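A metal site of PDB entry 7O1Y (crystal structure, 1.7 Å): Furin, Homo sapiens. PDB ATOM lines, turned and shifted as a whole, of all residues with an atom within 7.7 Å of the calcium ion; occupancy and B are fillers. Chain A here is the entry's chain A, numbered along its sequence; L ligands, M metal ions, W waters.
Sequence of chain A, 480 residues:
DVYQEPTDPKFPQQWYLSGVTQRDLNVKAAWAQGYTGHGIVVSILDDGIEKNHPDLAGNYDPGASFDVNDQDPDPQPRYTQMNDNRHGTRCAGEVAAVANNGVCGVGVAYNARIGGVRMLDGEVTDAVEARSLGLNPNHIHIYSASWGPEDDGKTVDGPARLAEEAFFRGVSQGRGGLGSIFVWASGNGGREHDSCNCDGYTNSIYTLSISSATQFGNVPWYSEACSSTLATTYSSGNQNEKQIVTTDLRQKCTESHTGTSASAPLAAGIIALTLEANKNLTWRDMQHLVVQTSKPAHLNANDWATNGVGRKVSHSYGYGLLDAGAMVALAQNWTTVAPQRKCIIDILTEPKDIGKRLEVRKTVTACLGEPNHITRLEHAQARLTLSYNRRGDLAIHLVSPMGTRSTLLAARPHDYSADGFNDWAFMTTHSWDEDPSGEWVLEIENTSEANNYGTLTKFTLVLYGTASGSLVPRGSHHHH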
ATOM      1  N   GLY A 148      21.553 -17.688 -22.033  1.00  0.00           N
ATOM      2  CA  GLY A 148      21.228 -17.636 -20.629  1.00  0.00           C
ATOM      3  C   GLY A 148      21.766 -18.862 -19.945  1.00  0.00           C
ATOM      4  O   GLY A 148      22.557 -19.626 -20.521  1.00  0.00           O
ATOM      5  N   PRO A 149      21.321 -19.113 -18.711  1.00  0.00           N
ATOM      6  CA  PRO A 149      21.889 -20.231 -17.952  1.00  0.00           C
ATOM      7  C   PRO A 149      21.595 -21.558 -18.637  1.00  0.00           C
ATOM      8  O   PRO A 149      20.637 -21.700 -19.386  1.00  0.00           O
ATOM      9  CB  PRO A 149      21.199 -20.134 -16.583  1.00  0.00           C
ATOM     10  CG  PRO A 149      19.961 -19.312 -16.822  1.00  0.00           C
ATOM     11  CD  PRO A 149      20.315 -18.367 -17.940  1.00  0.00           C
ATOM     12  N   GLU A 150      22.449 -22.536 -18.348  1.00  0.00           N
ATOM     13  CA  GLU A 150      22.289 -23.854 -18.969  1.00  0.00           C
ATOM     14  C   GLU A 150      20.873 -24.378 -18.771  1.00  0.00           C
ATOM     15  O   GLU A 150      20.290 -24.269 -17.677  1.00  0.00           O
ATOM     16  CB  GLU A 150      23.287 -24.847 -18.368  1.00  0.00           C
ATOM     17  CG  GLU A 150      24.766 -24.553 -18.733  1.00  0.00           C
ATOM     18  CD  GLU A 150      25.087 -24.637 -20.231  1.00  0.00           C
ATOM     19  OE1 GLU A 150      26.149 -24.101 -20.636  1.00  0.00           O
ATOM     20  OE2 GLU A 150      24.309 -25.234 -21.025  1.00  0.00           O
ATOM     21  N   ASP A 151      20.327 -24.952 -19.840  1.00  0.00           N
ATOM     22  CA  ASP A 151      18.982 -25.544 -19.830  1.00  0.00           C
ATOM     23  C   ASP A 151      19.059 -26.991 -19.338  1.00  0.00           C
ATOM     24  O   ASP A 151      18.557 -27.916 -19.975  1.00  0.00           O
ATOM     25  CB  ASP A 151      18.363 -25.474 -21.221  1.00  0.00           C
ATOM     26  CG  ASP A 151      17.922 -24.083 -21.598  1.00  0.00           C
ATOM     27  OD1 ASP A 151      17.589 -23.330 -20.662  1.00  0.00           O
ATOM     28  OD2 ASP A 151      17.851 -23.769 -22.810  1.00  0.00           O
ATOM     29  N   ASP A 152      19.705 -27.199 -18.201  1.00  0.00           N
ATOM     30  CA  ASP A 152      19.858 -28.535 -17.638  1.00  0.00           C
ATOM     31  C   ASP A 152      18.793 -28.905 -16.633  1.00  0.00           C
ATOM     32  O   ASP A 152      18.825 -30.028 -16.100  1.00  0.00           O
ATOM     33  CB  ASP A 152      21.252 -28.691 -16.992  1.00  0.00           C
ATOM     34  CG  ASP A 152      21.538 -27.650 -15.906  1.00  0.00           C
ATOM     35  OD1 ASP A 152      20.636 -26.894 -15.482  1.00  0.00           O
ATOM     36  OD2 ASP A 152      22.709 -27.584 -15.497  1.00  0.00           O
ATOM     37  N   GLY A 153      17.839 -28.011 -16.353  1.00  0.00           N
ATOM     38  CA  GLY A 153      16.800 -28.301 -15.402  1.00  0.00           C
ATOM     39  C   GLY A 153      17.237 -28.295 -13.959  1.00  0.00           C
ATOM     40  O   GLY A 153      16.499 -28.777 -13.105  1.00  0.00           O
ATOM     41  N   THR A 155      19.608 -25.443 -12.891  1.00  0.00           N
ATOM     42  CA  THR A 155      20.289 -24.181 -12.670  1.00  0.00           C
ATOM     43  C   THR A 155      19.269 -23.090 -12.377  1.00  0.00           C
ATOM     44  O   THR A 155      18.196 -23.060 -12.987  1.00  0.00           O
ATOM     45  CB  THR A 155      21.124 -23.805 -13.911  1.00  0.00           C
ATOM     46  OG1 THR A 155      22.092 -24.829 -14.176  1.00  0.00           O
ATOM     47  CG2 THR A 155      21.867 -22.514 -13.701  1.00  0.00           C
ATOM     48  N   ALA A 185      14.219 -15.703 -26.282  1.00  0.00           N
ATOM     49  CA  ALA A 185      13.671 -17.057 -26.289  1.00  0.00           C
ATOM     50  C   ALA A 185      13.548 -17.585 -24.867  1.00  0.00           C
ATOM     51  O   ALA A 185      14.439 -17.415 -24.041  1.00  0.00           O
ATOM     52  CB  ALA A 185      14.586 -17.951 -27.117  1.00  0.00           C
ATOM     53  N   SER A 186      12.445 -18.304 -24.577  1.00  0.00           N
ATOM     54  CA  SER A 186      12.203 -18.734 -23.197  1.00  0.00           C
ATOM     55  C   SER A 186      13.028 -19.962 -22.789  1.00  0.00           C
ATOM     56  O   SER A 186      12.983 -20.326 -21.601  1.00  0.00           O
ATOM     57  CB  SER A 186      10.730 -19.009 -22.997  1.00  0.00           C
ATOM     58  OG  SER A 186      10.262 -20.008 -23.907  1.00  0.00           O
ATOM     59  N   GLY A 187      13.766 -20.593 -23.699  1.00  0.00           N
ATOM     60  CA  GLY A 187      14.644 -21.708 -23.339  1.00  0.00           C
ATOM     61  C   GLY A 187      14.399 -22.946 -24.196  1.00  0.00           C
ATOM     62  O   GLY A 187      13.393 -23.091 -24.879  1.00  0.00           O
ATOM     63  N   ASN A 188      15.368 -23.878 -24.111  1.00  0.00           N
ATOM     64  CA  ASN A 188      15.323 -25.162 -24.833  1.00  0.00           C
ATOM     65  C   ASN A 188      15.419 -26.376 -23.912  1.00  0.00           C
ATOM     66  O   ASN A 188      15.795 -27.470 -24.372  1.00  0.00           O
ATOM     67  CB  ASN A 188      16.436 -25.219 -25.884  1.00  0.00           C
ATOM     68  CG  ASN A 188      16.103 -24.410 -27.130  1.00  0.00           C
ATOM     69  OD1 ASN A 188      15.019 -24.559 -27.688  1.00  0.00           O
ATOM     70  ND2 ASN A 188      17.013 -23.552 -27.552  1.00  0.00           N
ATOM     71  N   GLY A 189      15.064 -26.221 -22.635  1.00  0.00           N
ATOM     72  CA  GLY A 189      15.255 -27.257 -21.621  1.00  0.00           C
ATOM     73  C   GLY A 189      14.102 -28.226 -21.390  1.00  0.00           C
ATOM     74  O   GLY A 189      14.067 -28.918 -20.364  1.00  0.00           O
ATOM     75  N   GLY A 190      13.194 -28.343 -22.360  1.00  0.00           N
ATOM     76  CA  GLY A 190      12.013 -29.166 -22.169  1.00  0.00           C
ATOM     77  C   GLY A 190      12.332 -30.619 -21.836  1.00  0.00           C
ATOM     78  O   GLY A 190      11.642 -31.242 -21.020  1.00  0.00           O
ATOM     79  N   ASP A 194      12.879 -28.512 -17.534  1.00  0.00           N
ATOM     80  CA  ASP A 194      13.249 -27.191 -17.018  1.00  0.00           C
ATOM     81  C   ASP A 194      12.002 -26.314 -16.940  1.00  0.00           C
ATOM     82  O   ASP A 194      10.998 -26.549 -17.635  1.00  0.00           O
ATOM     83  CB  ASP A 194      14.317 -26.577 -17.921  1.00  0.00           C
ATOM     84  CG  ASP A 194      15.110 -25.477 -17.263  1.00  0.00           C
ATOM     85  OD1 ASP A 194      14.836 -25.105 -16.090  1.00  0.00           O
ATOM     86  OD2 ASP A 194      16.041 -24.961 -17.932  1.00  0.00           O
ATOM     87  N   SER A 195      12.065 -25.315 -16.059  1.00  0.00           N
ATOM     88  CA  SER A 195      10.937 -24.440 -15.736  1.00  0.00           C
ATOM     89  C   SER A 195      11.487 -23.016 -15.849  1.00  0.00           C
ATOM     90  O   SER A 195      12.359 -22.648 -15.075  1.00  0.00           O
ATOM     91  CB  SER A 195      10.432 -24.783 -14.334  1.00  0.00           C
ATOM     92  OG  SER A 195       9.266 -24.117 -13.904  1.00  0.00           O
ATOM     93  N   CYS A 196      11.016 -22.228 -16.841  1.00  0.00           N
ATOM     94  CA  CYS A 196      11.867 -21.142 -17.312  1.00  0.00           C
ATOM     95  C   CYS A 196      11.858 -19.886 -16.441  1.00  0.00           C
ATOM     96  O   CYS A 196      12.643 -18.970 -16.718  1.00  0.00           O
ATOM     97  CB  CYS A 196      11.548 -20.753 -18.778  1.00  0.00           C
ATOM     98  SG  CYS A 196       9.787 -20.783 -19.400  1.00  0.00           S
ATOM     99  N   ASN A 197      11.029 -19.790 -15.385  1.00  0.00           N
ATOM    100  CA  ASN A 197      11.255 -18.644 -14.512  1.00  0.00           C
ATOM    101  C   ASN A 197      12.576 -18.753 -13.766  1.00  0.00           C
ATOM    102  O   ASN A 197      12.993 -17.771 -13.135  1.00  0.00           O
ATOM    103  CB  ASN A 197      10.147 -18.433 -13.468  1.00  0.00           C
ATOM    104  CG  ASN A 197       8.811 -18.035 -14.071  1.00  0.00           C
ATOM    105  OD1 ASN A 197       8.725 -17.554 -15.195  1.00  0.00           O
ATOM    106  ND2 ASN A 197       7.748 -18.199 -13.293  1.00  0.00           N
ATOM    107  N   CYS A 198      13.212 -19.923 -13.783  1.00  0.00           N
ATOM    108  CA  CYS A 198      14.558 -20.102 -13.218  1.00  0.00           C
ATOM    109  C   CYS A 198      15.643 -19.503 -14.082  1.00  0.00           C
ATOM    110  O   CYS A 198      16.832 -19.611 -13.731  1.00  0.00           O
ATOM    111  CB  CYS A 198      14.828 -21.592 -13.032  1.00  0.00           C
ATOM    112  SG  CYS A 198      13.804 -22.317 -11.725  1.00  0.00           S
ATOM    113  N   ASP A 199      15.277 -18.921 -15.223  1.00  0.00           N
ATOM    114  CA  ASP A 199      16.176 -18.233 -16.153  1.00  0.00           C
ATOM    115  C   ASP A 199      15.883 -16.746 -16.045  1.00  0.00           C
ATOM    116  O   ASP A 199      14.842 -16.275 -16.523  1.00  0.00           O
ATOM    117  CB  ASP A 199      15.950 -18.794 -17.551  1.00  0.00           C
ATOM    118  CG  ASP A 199      16.583 -17.969 -18.680  1.00  0.00           C
ATOM    119  OD1 ASP A 199      17.112 -16.866 -18.476  1.00  0.00           O
ATOM    120  OD2 ASP A 199      16.497 -18.457 -19.827  1.00  0.00           O
ATOM    121  N   THR A 202      14.962 -14.534 -19.394  1.00  0.00           N
ATOM    122  CA  THR A 202      13.580 -14.586 -19.890  1.00  0.00           C
ATOM    123  C   THR A 202      12.593 -14.178 -18.812  1.00  0.00           C
ATOM    124  O   THR A 202      11.544 -13.587 -19.115  1.00  0.00           O
ATOM    125  CB  THR A 202      13.280 -15.983 -20.469  1.00  0.00           C
ATOM    126  OG1 THR A 202      12.091 -15.930 -21.274  1.00  0.00           O
ATOM    127  CG2 THR A 202      13.110 -17.064 -19.393  1.00  0.00           C
ATOM    128  N   TYR A 222      11.232 -29.498 -26.816  1.00  0.00           N
ATOM    129  CA  TYR A 222      12.238 -28.637 -26.184  1.00  0.00           C
ATOM    130  C   TYR A 222      11.648 -27.486 -25.362  1.00  0.00           C
ATOM    131  O   TYR A 222      12.400 -26.774 -24.688  1.00  0.00           O
ATOM    132  CB  TYR A 222      13.195 -28.055 -27.238  1.00  0.00           C
ATOM    133  CG  TYR A 222      12.484 -27.435 -28.390  1.00  0.00           C
ATOM    134  CD1 TYR A 222      11.968 -26.161 -28.315  1.00  0.00           C
ATOM    135  CD2 TYR A 222      12.323 -28.145 -29.597  1.00  0.00           C
ATOM    136  CE1 TYR A 222      11.278 -25.594 -29.369  1.00  0.00           C
ATOM    137  CE2 TYR A 222      11.619 -27.596 -30.661  1.00  0.00           C
ATOM    138  CZ  TYR A 222      11.109 -26.304 -30.544  1.00  0.00           C
ATOM    139  OH  TYR A 222      10.404 -25.679 -31.551  1.00  0.00           O
ATOM    140  N   GLU A 224       9.991 -24.979 -22.642  1.00  0.00           N
ATOM    141  CA  GLU A 224       9.852 -24.800 -21.200  1.00  0.00           C
ATOM    142  C   GLU A 224       8.612 -23.983 -20.930  1.00  0.00           C
ATOM    143  O   GLU A 224       8.382 -22.965 -21.601  1.00  0.00           O
ATOM    144  CB  GLU A 224      11.065 -24.087 -20.594  1.00  0.00           C
ATOM    145  CG  GLU A 224      12.405 -24.830 -20.835  1.00  0.00           C
ATOM    146  CD  GLU A 224      13.604 -24.052 -20.257  1.00  0.00           C
ATOM    147  OE1 GLU A 224      14.676 -24.020 -20.937  1.00  0.00           O
ATOM    148  OE2 GLU A 224      13.486 -23.503 -19.134  1.00  0.00           O
ATOM    149  N   ARG A 412      11.153 -29.582 -10.629  1.00  0.00           N
ATOM    150  CA  ARG A 412      12.268 -29.854 -11.542  1.00  0.00           C
ATOM    151  C   ARG A 412      13.019 -31.066 -11.017  1.00  0.00           C
ATOM    152  O   ARG A 412      13.795 -30.969 -10.044  1.00  0.00           O
ATOM    153  CB  ARG A 412      13.203 -28.648 -11.665  1.00  0.00           C
ATOM    154  CG  ARG A 412      12.572 -27.458 -12.357  1.00  0.00           C
ATOM    155  CD  ARG A 412      13.628 -26.511 -12.920  1.00  0.00           C
ATOM    156  NE  ARG A 412      14.556 -26.013 -11.900  1.00  0.00           N
ATOM    157  CZ  ARG A 412      15.686 -25.372 -12.174  1.00  0.00           C
ATOM    158  NH1 ARG A 412      16.477 -24.992 -11.163  1.00  0.00           N
ATOM    159  NH2 ARG A 412      16.010 -25.105 -13.433  1.00  0.00           N
HETATM  160  N1  LIG L   1      25.163 -19.987 -30.961  1.00  0.00           N
HETATM  161  C1  LIG L   1      19.160 -20.251 -21.969  1.00  0.00           C
HETATM  162  C2  LIG L   1      23.836 -22.884 -24.472  1.00  0.00           C
HETATM  163  N2  LIG L   1      26.168 -21.755 -29.890  1.00  0.00           N
HETATM  164  C3  LIG L   1      24.649 -23.031 -25.580  1.00  0.00           C
HETATM  165  C4  LIG L   1      25.396 -22.323 -27.844  1.00  0.00           C
HETATM  166  C5  LIG L   1      22.868 -21.882 -24.412  1.00  0.00           C
HETATM  167  C6  LIG L   1      21.940 -21.824 -23.282  1.00  0.00           C
HETATM  168  N3  LIG L   1      25.289 -21.540 -28.845  1.00  0.00           N
HETATM  169  C7  LIG L   1      22.745 -21.037 -25.513  1.00  0.00           C
HETATM  170  C8  LIG L   1      23.558 -21.184 -26.622  1.00  0.00           C
HETATM  171  C9  LIG L   1      24.523 -22.182 -26.673  1.00  0.00           C
HETATM  172  N4  LIG L   1      20.921 -21.049 -23.282  1.00  0.00           N
HETATM  173  N5  LIG L   1      26.891 -21.115 -31.982  1.00  0.00           N
HETATM  174  C10 LIG L   1      26.068 -20.942 -30.953  1.00  0.00           C
HETATM  175  N6  LIG L   1      20.254 -21.030 -22.079  1.00  0.00           N
HETATM  176  N7  LIG L   1      18.697 -19.621 -23.031  1.00  0.00           N
HETATM  177  N8  LIG L   1      18.640 -20.054 -20.785  1.00  0.00           N
HETATM  178 CA    CA M   1      15.843 -22.902 -19.136  1.00  0.00          CA
HETATM  179  O   HOH W   1      15.228 -22.324 -16.743  1.00  0.00           O
HETATM  180  O   HOH W   2      17.934 -22.118 -18.117  1.00  0.00           O
HETATM  181  O   HOH W   3      15.029 -20.867 -19.977  1.00  0.00           O
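Water W3 lies within hydrogen-bond range of the backbone carbonyl oxygen of Ser 186 (2.7 Å) and the side-chain carboxylate of Asp 199 (2.8 Å).
Water W2 lies within hydrogen-bond range of the backbone carbonyl oxygen of Pro 149 (3.0 Å), the backbone carbonyl oxygen of Glu 150 (3.2 Å) and a nitrogen (N8) of the ligand (3.4 Å).
Water W1 bridges OD1 of Asp 194 (2.9 Å) and O of Ser 195 (3.3 Å).
OD1 of Asp 151 sits close to N8 of the ligand (3.4 Å).
The side-chain carboxylate (OD2) of Asp 199 lies within salt-bridge range of a nitrogen (N8) of the ligand.
The backbone carbonyl oxygen (O) of Pro 149 is in hydrogen-bond range of a nitrogen (N8) of the ligand (2.9 Å).
O of Gly 148 lies close to N6 of the ligand.
The nearest printed residue that does not touch the calcium ion is Asp 199 (4.4 Å).
The calcium ion is bound by water W3 (2.3 Å), the side-chain carboxylate (OD1) of Asp 151 (2.4 Å), the side-chain carboxylate (OD2) of Asp 194 (2.4 Å), the side-chain carboxylate (OE1) of Glu 224 (2.4 Å), the side-chain carboxylate (OE2) of Glu 224 (2.4 Å), water W2 (2.5 Å) and water W1 (2.5 Å).
N of Asn 188 lies within hydrogen-bond range of OD2 of Asp 151 (2.8 Å).
N of Asp 194 sits at hydrogen-bond distance from O of Gly 189 (3.1 Å).
NH2 of Arg 412 is in salt-bridge range of OD1 of Asp 194.
The backbone NH (N) of Gly 189 lies close to the side-chain carboxylate (OE1) of Glu 224, at 2.8 Å.
The backbone NH (N) of Asn 188 lies close to the side-chain carboxylate (OE1) of Glu 224 (3.3 Å).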
